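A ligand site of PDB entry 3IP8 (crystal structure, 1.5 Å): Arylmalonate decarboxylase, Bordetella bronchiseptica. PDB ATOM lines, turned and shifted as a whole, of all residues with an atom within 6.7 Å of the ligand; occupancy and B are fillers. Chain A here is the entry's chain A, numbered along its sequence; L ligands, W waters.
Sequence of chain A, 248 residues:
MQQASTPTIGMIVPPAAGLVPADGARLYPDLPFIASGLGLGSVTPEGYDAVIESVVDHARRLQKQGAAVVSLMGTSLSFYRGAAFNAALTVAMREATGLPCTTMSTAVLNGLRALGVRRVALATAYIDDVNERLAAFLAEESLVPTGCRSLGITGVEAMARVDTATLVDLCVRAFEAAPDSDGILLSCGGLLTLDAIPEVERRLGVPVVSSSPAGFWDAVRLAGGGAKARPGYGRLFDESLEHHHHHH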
ATOM      1  N   VAL A  13      -1.304  24.399   3.166  1.00  0.00           N
ATOM      2  CA  VAL A  13      -2.724  24.067   3.134  1.00  0.00           C
ATOM      3  C   VAL A  13      -3.096  23.417   1.819  1.00  0.00           C
ATOM      4  O   VAL A  13      -2.532  23.741   0.787  1.00  0.00           O
ATOM      5  CB  VAL A  13      -3.593  25.323   3.366  1.00  0.00           C
ATOM      6  CG1 VAL A  13      -3.305  25.931   4.734  1.00  0.00           C
ATOM      7  CG2 VAL A  13      -3.375  26.379   2.264  1.00  0.00           C
ATOM      8  N   PRO A  14      -4.054  22.492   1.817  1.00  0.00           N
ATOM      9  CA  PRO A  14      -4.443  21.832   0.576  1.00  0.00           C
ATOM     10  C   PRO A  14      -4.952  22.730  -0.572  1.00  0.00           C
ATOM     11  O   PRO A  14      -4.519  22.515  -1.692  1.00  0.00           O
ATOM     12  CB  PRO A  14      -5.487  20.801   1.028  1.00  0.00           C
ATOM     13  CG  PRO A  14      -4.999  20.419   2.416  1.00  0.00           C
ATOM     14  CD  PRO A  14      -4.533  21.754   3.012  1.00  0.00           C
ATOM     15  N   PRO A  15      -5.839  23.714  -0.303  1.00  0.00           N
ATOM     16  CA  PRO A  15      -6.396  24.451  -1.458  1.00  0.00           C
ATOM     17  C   PRO A  15      -5.415  25.350  -2.187  1.00  0.00           C
ATOM     18  O   PRO A  15      -4.495  25.893  -1.576  1.00  0.00           O
ATOM     19  CB  PRO A  15      -7.516  25.293  -0.832  1.00  0.00           C
ATOM     20  CG  PRO A  15      -7.854  24.566   0.476  1.00  0.00           C
ATOM     21  CD  PRO A  15      -6.495  24.085   0.957  1.00  0.00           C
ATOM     22  N   LEU A  40      -4.413  20.909  -4.098  1.00  0.00           N
ATOM     23  CA  LEU A  40      -5.028  19.587  -4.093  1.00  0.00           C
ATOM     24  C   LEU A  40      -6.312  19.620  -4.935  1.00  0.00           C
ATOM     25  O   LEU A  40      -7.159  20.503  -4.753  1.00  0.00           O
ATOM     26  CB  LEU A  40      -5.344  19.174  -2.658  1.00  0.00           C
ATOM     27  CG  LEU A  40      -6.013  17.809  -2.455  1.00  0.00           C
ATOM     28  CD1 LEU A  40      -5.100  16.669  -2.926  1.00  0.00           C
ATOM     29  CD2 LEU A  40      -6.345  17.616  -0.981  1.00  0.00           C
ATOM     30  N   VAL A  43     -10.077  15.099  -2.512  1.00  0.00           N
ATOM     31  CA  VAL A  43      -9.770  14.496  -1.224  1.00  0.00           C
ATOM     32  C   VAL A  43      -9.861  12.996  -1.426  1.00  0.00           C
ATOM     33  O   VAL A  43     -10.769  12.325  -0.940  1.00  0.00           O
ATOM     34  CB  VAL A  43     -10.729  15.021  -0.132  1.00  0.00           C
ATOM     35  CG1 VAL A  43     -10.294  14.493   1.233  1.00  0.00           C
ATOM     36  CG2 VAL A  43     -10.704  16.550  -0.103  1.00  0.00           C
ATOM     37  N   TYR A  48      -4.078  13.072  -3.508  1.00  0.00           N
ATOM     38  CA  TYR A  48      -2.905  13.348  -2.681  1.00  0.00           C
ATOM     39  C   TYR A  48      -1.604  13.073  -3.442  1.00  0.00           C
ATOM     40  O   TYR A  48      -0.658  13.833  -3.325  1.00  0.00           O
ATOM     41  CB  TYR A  48      -2.888  12.494  -1.410  1.00  0.00           C
ATOM     42  CG  TYR A  48      -4.197  12.452  -0.677  1.00  0.00           C
ATOM     43  CD1 TYR A  48      -4.969  13.601  -0.522  1.00  0.00           C
ATOM     44  CD2 TYR A  48      -4.677  11.259  -0.158  1.00  0.00           C
ATOM     45  CE1 TYR A  48      -6.195  13.542   0.142  1.00  0.00           C
ATOM     46  CE2 TYR A  48      -5.887  11.205   0.500  1.00  0.00           C
ATOM     47  CZ  TYR A  48      -6.639  12.345   0.650  1.00  0.00           C
ATOM     48  OH  TYR A  48      -7.863  12.237   1.293  1.00  0.00           O
ATOM     49  N   MET A  73      -0.936  21.339   7.098  1.00  0.00           N
ATOM     50  CA  MET A  73      -2.307  21.398   7.599  1.00  0.00           C
ATOM     51  C   MET A  73      -3.255  20.602   6.703  1.00  0.00           C
ATOM     52  O   MET A  73      -4.239  21.125   6.174  1.00  0.00           O
ATOM     53  CB  MET A  73      -2.721  22.861   7.749  1.00  0.00           C
ATOM     54  CG  MET A  73      -1.920  23.565   8.861  1.00  0.00           C
ATOM     55  SD  MET A  73      -2.530  23.141  10.528  1.00  0.00           S
ATOM     56  CE  MET A  73      -4.087  24.077  10.562  1.00  0.00           C
ATOM     57  N   GLY A  74      -2.940  19.324   6.559  1.00  0.00           N
ATOM     58  CA  GLY A  74      -3.818  18.401   5.858  1.00  0.00           C
ATOM     59  C   GLY A  74      -3.808  17.094   6.627  1.00  0.00           C
ATOM     60  O   GLY A  74      -2.726  16.586   6.893  1.00  0.00           O
ATOM     61  N   THR A  75      -4.976  16.605   7.029  1.00  0.00           N
ATOM     62  CA  THR A  75      -5.083  15.354   7.783  1.00  0.00           C
ATOM     63  C   THR A  75      -4.854  14.141   6.854  1.00  0.00           C
ATOM     64  O   THR A  75      -3.878  13.391   6.997  1.00  0.00           O
ATOM     65  CB  THR A  75      -6.450  15.230   8.497  1.00  0.00           C
ATOM     66  OG1 THR A  75      -6.959  16.550   8.745  1.00  0.00           O
ATOM     67  CG2 THR A  75      -6.299  14.499   9.825  1.00  0.00           C
ATOM     68  N   SER A  76      -5.739  13.964   5.877  1.00  0.00           N
ATOM     69  CA  SER A  76      -5.620  12.803   5.025  1.00  0.00           C
ATOM     70  C   SER A  76      -4.364  12.838   4.181  1.00  0.00           C
ATOM     71  O   SER A  76      -3.790  11.802   3.932  1.00  0.00           O
ATOM     72  CB  SER A  76      -6.873  12.589   4.166  1.00  0.00           C
ATOM     73  OG  SER A  76      -7.214  13.769   3.463  1.00  0.00           O
ATOM     74  N   LEU A  77      -3.897  14.014   3.764  1.00  0.00           N
ATOM     75  CA  LEU A  77      -2.605  14.100   3.075  1.00  0.00           C
ATOM     76  C   LEU A  77      -1.472  13.504   3.880  1.00  0.00           C
ATOM     77  O   LEU A  77      -0.498  12.977   3.315  1.00  0.00           O
ATOM     78  CB  LEU A  77      -2.273  15.574   2.793  1.00  0.00           C
ATOM     79  CG  LEU A  77      -2.671  16.077   1.421  1.00  0.00           C
ATOM     80  CD1 LEU A  77      -2.519  17.587   1.376  1.00  0.00           C
ATOM     81  CD2 LEU A  77      -1.847  15.394   0.350  1.00  0.00           C
ATOM     82  N   SER A  78      -1.574  13.615   5.200  1.00  0.00           N
ATOM     83  CA  SER A  78      -0.522  13.103   6.068  1.00  0.00           C
ATOM     84  C   SER A  78      -0.760  11.710   6.635  1.00  0.00           C
ATOM     85  O   SER A  78       0.198  11.060   7.068  1.00  0.00           O
ATOM     86  CB  SER A  78      -0.124  14.113   7.178  1.00  0.00           C
ATOM     87  OG  SER A  78      -1.231  14.549   7.989  1.00  0.00           O
ATOM     88  N   PHE A  79      -2.014  11.231   6.631  1.00  0.00           N
ATOM     89  CA  PHE A  79      -2.271   9.879   7.161  1.00  0.00           C
ATOM     90  C   PHE A  79      -2.490   8.769   6.116  1.00  0.00           C
ATOM     91  O   PHE A  79      -2.501   7.580   6.447  1.00  0.00           O
ATOM     92  CB  PHE A  79      -3.380   9.848   8.245  1.00  0.00           C
ATOM     93  CG  PHE A  79      -4.790  10.044   7.731  1.00  0.00           C
ATOM     94  CD1 PHE A  79      -5.376   9.182   6.819  1.00  0.00           C
ATOM     95  CD2 PHE A  79      -5.551  11.091   8.250  1.00  0.00           C
ATOM     96  CE1 PHE A  79      -6.671   9.399   6.366  1.00  0.00           C
ATOM     97  CE2 PHE A  79      -6.825  11.305   7.821  1.00  0.00           C
ATOM     98  CZ  PHE A  79      -7.404  10.469   6.876  1.00  0.00           C
ATOM     99  N   MET A 104      -0.972  17.896  10.439  1.00  0.00           N
ATOM    100  CA  MET A 104      -2.303  17.857  11.033  1.00  0.00           C
ATOM    101  C   MET A 104      -2.661  16.453  11.574  1.00  0.00           C
ATOM    102  O   MET A 104      -3.449  16.336  12.536  1.00  0.00           O
ATOM    103  CB  MET A 104      -3.301  18.352   9.985  1.00  0.00           C
ATOM    104  CG  MET A 104      -4.726  18.514  10.476  1.00  0.00           C
ATOM    105  SD  MET A 104      -5.756  19.317   9.213  1.00  0.00           S
ATOM    106  CE  MET A 104      -5.473  21.025   9.636  1.00  0.00           C
ATOM    107  N   TYR A 126     -15.218  12.317   4.650  1.00  0.00           N
ATOM    108  CA  TYR A 126     -14.546  11.578   3.561  1.00  0.00           C
ATOM    109  C   TYR A 126     -15.328  10.433   2.967  1.00  0.00           C
ATOM    110  O   TYR A 126     -16.289   9.953   3.564  1.00  0.00           O
ATOM    111  CB  TYR A 126     -13.235  10.966   4.043  1.00  0.00           C
ATOM    112  CG  TYR A 126     -12.309  11.874   4.819  1.00  0.00           C
ATOM    113  CD1 TYR A 126     -11.906  13.112   4.301  1.00  0.00           C
ATOM    114  CD2 TYR A 126     -11.746  11.445   6.008  1.00  0.00           C
ATOM    115  CE1 TYR A 126     -11.011  13.926   5.030  1.00  0.00           C
ATOM    116  CE2 TYR A 126     -10.861  12.250   6.736  1.00  0.00           C
ATOM    117  CZ  TYR A 126     -10.504  13.481   6.228  1.00  0.00           C
ATOM    118  OH  TYR A 126      -9.620  14.280   6.926  1.00  0.00           O
ATOM    119  N   VAL A 130     -10.802   6.584   2.214  1.00  0.00           N
ATOM    120  CA  VAL A 130     -10.046   7.482   3.079  1.00  0.00           C
ATOM    121  C   VAL A 130     -10.356   7.179   4.557  1.00  0.00           C
ATOM    122  O   VAL A 130      -9.454   7.193   5.395  1.00  0.00           O
ATOM    123  CB  VAL A 130     -10.277   8.981   2.702  1.00  0.00           C
ATOM    124  CG1 VAL A 130      -9.504   9.888   3.626  1.00  0.00           C
ATOM    125  CG2 VAL A 130      -9.862   9.239   1.251  1.00  0.00           C
ATOM    126  N   GLY A 155     -14.695  16.935  -2.865  1.00  0.00           N
ATOM    127  CA  GLY A 155     -14.319  18.294  -3.219  1.00  0.00           C
ATOM    128  C   GLY A 155     -13.469  18.902  -2.124  1.00  0.00           C
ATOM    129  O   GLY A 155     -13.725  18.670  -0.935  1.00  0.00           O
ATOM    130  N   VAL A 156     -12.456  19.670  -2.509  1.00  0.00           N
ATOM    131  CA  VAL A 156     -11.543  20.298  -1.568  1.00  0.00           C
ATOM    132  C   VAL A 156     -12.132  21.621  -1.037  1.00  0.00           C
ATOM    133  O   VAL A 156     -12.406  21.773   0.161  1.00  0.00           O
ATOM    134  CB  VAL A 156     -10.192  20.562  -2.237  1.00  0.00           C
ATOM    135  CG1 VAL A 156      -9.279  21.361  -1.313  1.00  0.00           C
ATOM    136  CG2 VAL A 156      -9.550  19.247  -2.656  1.00  0.00           C
ATOM    137  N   GLU A 157     -12.343  22.570  -1.922  1.00  0.00           N
ATOM    138  CA  GLU A 157     -12.922  23.845  -1.522  1.00  0.00           C
ATOM    139  C   GLU A 157     -14.360  23.671  -1.016  1.00  0.00           C
ATOM    140  O   GLU A 157     -14.838  24.453  -0.186  1.00  0.00           O
ATOM    141  CB  GLU A 157     -12.839  24.831  -2.695  1.00  0.00           C
ATOM    142  CG  GLU A 157     -11.406  25.357  -2.985  1.00  0.00           C
ATOM    143  CD  GLU A 157     -10.516  24.387  -3.775  1.00  0.00           C
ATOM    144  OE1 GLU A 157     -10.988  23.339  -4.298  1.00  0.00           O
ATOM    145  OE2 GLU A 157      -9.313  24.697  -3.888  1.00  0.00           O
ATOM    146  N   MET A 159     -15.499  21.717   1.053  1.00  0.00           N
ATOM    147  CA  MET A 159     -15.565  21.426   2.496  1.00  0.00           C
ATOM    148  C   MET A 159     -16.012  22.614   3.314  1.00  0.00           C
ATOM    149  O   MET A 159     -16.726  22.472   4.305  1.00  0.00           O
ATOM    150  CB  MET A 159     -14.186  20.935   2.988  1.00  0.00           C
ATOM    151  CG  MET A 159     -13.720  19.617   2.415  1.00  0.00           C
ATOM    152  SD  MET A 159     -14.836  18.248   2.778  1.00  0.00           S
ATOM    153  CE  MET A 159     -13.908  16.911   2.015  1.00  0.00           C
ATOM    154  N   ALA A 160     -15.623  23.826   2.904  1.00  0.00           N
ATOM    155  CA  ALA A 160     -15.896  25.013   3.714  1.00  0.00           C
ATOM    156  C   ALA A 160     -17.383  25.332   3.792  1.00  0.00           C
ATOM    157  O   ALA A 160     -17.815  26.095   4.650  1.00  0.00           O
ATOM    158  CB  ALA A 160     -15.112  26.199   3.153  1.00  0.00           C
ATOM    159  N   SER A 187     -12.835  14.763  11.467  1.00  0.00           N
ATOM    160  CA  SER A 187     -11.707  14.869  10.568  1.00  0.00           C
ATOM    161  C   SER A 187     -12.096  15.495   9.263  1.00  0.00           C
ATOM    162  O   SER A 187     -13.042  15.051   8.606  1.00  0.00           O
ATOM    163  CB  SER A 187     -11.104  13.488  10.317  1.00  0.00           C
ATOM    164  OG  SER A 187      -9.802  13.587   9.692  1.00  0.00           O
ATOM    165  N   CYS A 188     -11.297  16.509   8.915  1.00  0.00           N
ATOM    166  CA  CYS A 188     -11.213  17.243   7.649  1.00  0.00           C
ATOM    167  C   CYS A 188     -10.947  18.711   7.950  1.00  0.00           C
ATOM    168  O   CYS A 188     -11.766  19.420   8.543  1.00  0.00           O
ATOM    169  CB  CYS A 188     -12.417  17.076   6.713  1.00  0.00           C
ATOM    170  SG  CYS A 188     -12.209  18.124   5.246  1.00  0.00           S
ATOM    171  N   GLY A 189      -9.753  19.131   7.585  1.00  0.00           N
ATOM    172  CA  GLY A 189      -9.291  20.454   7.908  1.00  0.00           C
ATOM    173  C   GLY A 189      -9.913  21.536   7.048  1.00  0.00           C
ATOM    174  O   GLY A 189      -9.629  22.706   7.264  1.00  0.00           O
ATOM    175  N   GLY A 190     -10.769  21.159   6.109  1.00  0.00           N
ATOM    176  CA  GLY A 190     -11.465  22.150   5.305  1.00  0.00           C
ATOM    177  C   GLY A 190     -12.806  22.527   5.905  1.00  0.00           C
ATOM    178  O   GLY A 190     -13.451  23.491   5.506  1.00  0.00           O
ATOM    179  N   LEU A 191     -13.235  21.759   6.896  1.00  0.00           N
ATOM    180  CA  LEU A 191     -14.524  22.052   7.537  1.00  0.00           C
ATOM    181  C   LEU A 191     -14.406  23.229   8.492  1.00  0.00           C
ATOM    182  O   LEU A 191     -13.355  23.426   9.086  1.00  0.00           O
ATOM    183  CB  LEU A 191     -14.993  20.842   8.346  1.00  0.00           C
ATOM    184  CG  LEU A 191     -15.175  19.532   7.577  1.00  0.00           C
ATOM    185  CD1 LEU A 191     -15.452  18.389   8.532  1.00  0.00           C
ATOM    186  CD2 LEU A 191     -16.323  19.701   6.602  1.00  0.00           C
ATOM    187  N   SER A 211      -9.871  18.477  13.116  1.00  0.00           N
ATOM    188  CA  SER A 211      -8.655  18.697  12.320  1.00  0.00           C
ATOM    189  C   SER A 211      -8.062  20.105  12.367  1.00  0.00           C
ATOM    190  O   SER A 211      -6.894  20.276  12.753  1.00  0.00           O
ATOM    191  CB  SER A 211      -8.890  18.354  10.838  1.00  0.00           C
ATOM    192  OG  SER A 211      -9.022  16.951  10.677  1.00  0.00           O
ATOM    193  N   SER A 212      -8.840  21.119  11.975  1.00  0.00           N
ATOM    194  CA  SER A 212      -8.264  22.460  11.850  1.00  0.00           C
ATOM    195  C   SER A 212      -7.923  23.047  13.206  1.00  0.00           C
ATOM    196  O   SER A 212      -6.772  23.468  13.424  1.00  0.00           O
ATOM    197  CB  SER A 212      -9.159  23.389  11.038  1.00  0.00           C
ATOM    198  OG  SER A 212      -8.447  24.576  10.702  1.00  0.00           O
HETATM  199  C1  LIG L   1      -9.750  19.645   2.654  1.00  0.00           C
HETATM  200  C2  LIG L   1      -9.781  21.040   2.366  1.00  0.00           C
HETATM  201  C3  LIG L   1      -8.928  21.892   3.021  1.00  0.00           C
HETATM  202  C4  LIG L   1      -7.982  21.391   4.038  1.00  0.00           C
HETATM  203  C5  LIG L   1      -7.955  20.039   4.335  1.00  0.00           C
HETATM  204  C6  LIG L   1      -8.851  19.163   3.643  1.00  0.00           C
HETATM  205  C7  LIG L   1      -8.982  17.677   3.951  1.00  0.00           C
HETATM  206  P1  LIG L   1      -7.805  16.906   5.131  1.00  0.00           P
HETATM  207  O1  LIG L   1      -7.919  17.542   6.593  1.00  0.00           O
HETATM  208  O2  LIG L   1      -8.023  15.310   5.187  1.00  0.00           O
HETATM  209  O3  LIG L   1      -6.439  17.143   4.599  1.00  0.00           O
HETATM  210  O   HOH W   1      -5.569  16.072   2.592  1.00  0.00           O
HETATM  211  O   HOH W   2      -7.197  24.724   4.181  1.00  0.00           O
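An oxygen (O1) of the ligand sits at hydrogen-bond distance from the side-chain hydroxyl (OG1) of Thr 75. The backbone NH of Ser 76 sits at hydrogen-bond distance from an oxygen (O2) of the ligand (2.7 Å). N of Thr 75 is in hydrogen-bond range of O3 of the ligand, at 2.9 Å. An oxygen (O1) of the ligand is in hydrogen-bond range of the backbone NH of Gly 189 (2.6 Å). OG of Ser 76 is in hydrogen-bond range of O2 of the ligand (2.4 Å). OH of Tyr 126 lies within hydrogen-bond range of O2 of the ligand.
OH of Tyr 126 sits at hydrogen-bond distance from N of Cys 188, at 3.4 Å. The side-chain hydroxyl (OG) of Ser 76 sits at hydrogen-bond distance from the side-chain hydroxyl (OH) of Tyr 48, 2.7 Å away. The backbone NH (N) of Gly 190 sits close to the side-chain sulfur (SG) of Cys 188, 3.5 Å away. OG of Ser 187 lies within hydrogen-bond range of OH of Tyr 126 (2.9 Å). The side-chain hydroxyl (OG) of Ser 211 lies within hydrogen-bond range of the side-chain hydroxyl (OG1) of Thr 75, 2.9 Å away. The backbone carbonyl oxygen (O) of Pro 14 lies within hydrogen-bond range of the backbone NH (N) of Leu 40 (2.9 Å). N of Cys 188 lies within hydrogen-bond range of OG of Ser 211, 2.9 Å away. The side-chain hydroxyl (OG1) of Thr 75 lies within hydrogen-bond range of the side-chain sulfur (SD) of Met 104 (3.1 Å).
Merely in contact with the ligand: Gly 74, Gly 190, Cys 188, Val 156, Pro 14, Met 104, Pro 15 and Met 159. Hydrophobic or aromatic side chains within 4 Å of the ligand: Pro 14, Pro 15, Met 104, Tyr 126, Val 156 and Met 159. 12 residues have an atom within 4 Å of the ligand: Pro 14, Pro 15, Gly 74, Thr 75, Ser 76, Met 104, Tyr 126, Val 156, Met 159, Cys 188, Gly 189 and Gly 190. Along chain A the residues within 4 Å of the ligand span positions 14 to 190. The nearest printed residue that does not touch the ligand is Leu 77 (4.1 Å).
Water W1 lies within hydrogen-bond range of an oxygen (O3) of the ligand (2.4 Å), the backbone NH of Leu 77 (2.9 Å) and the side-chain hydroxyl of Ser 76 (3.0 Å).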
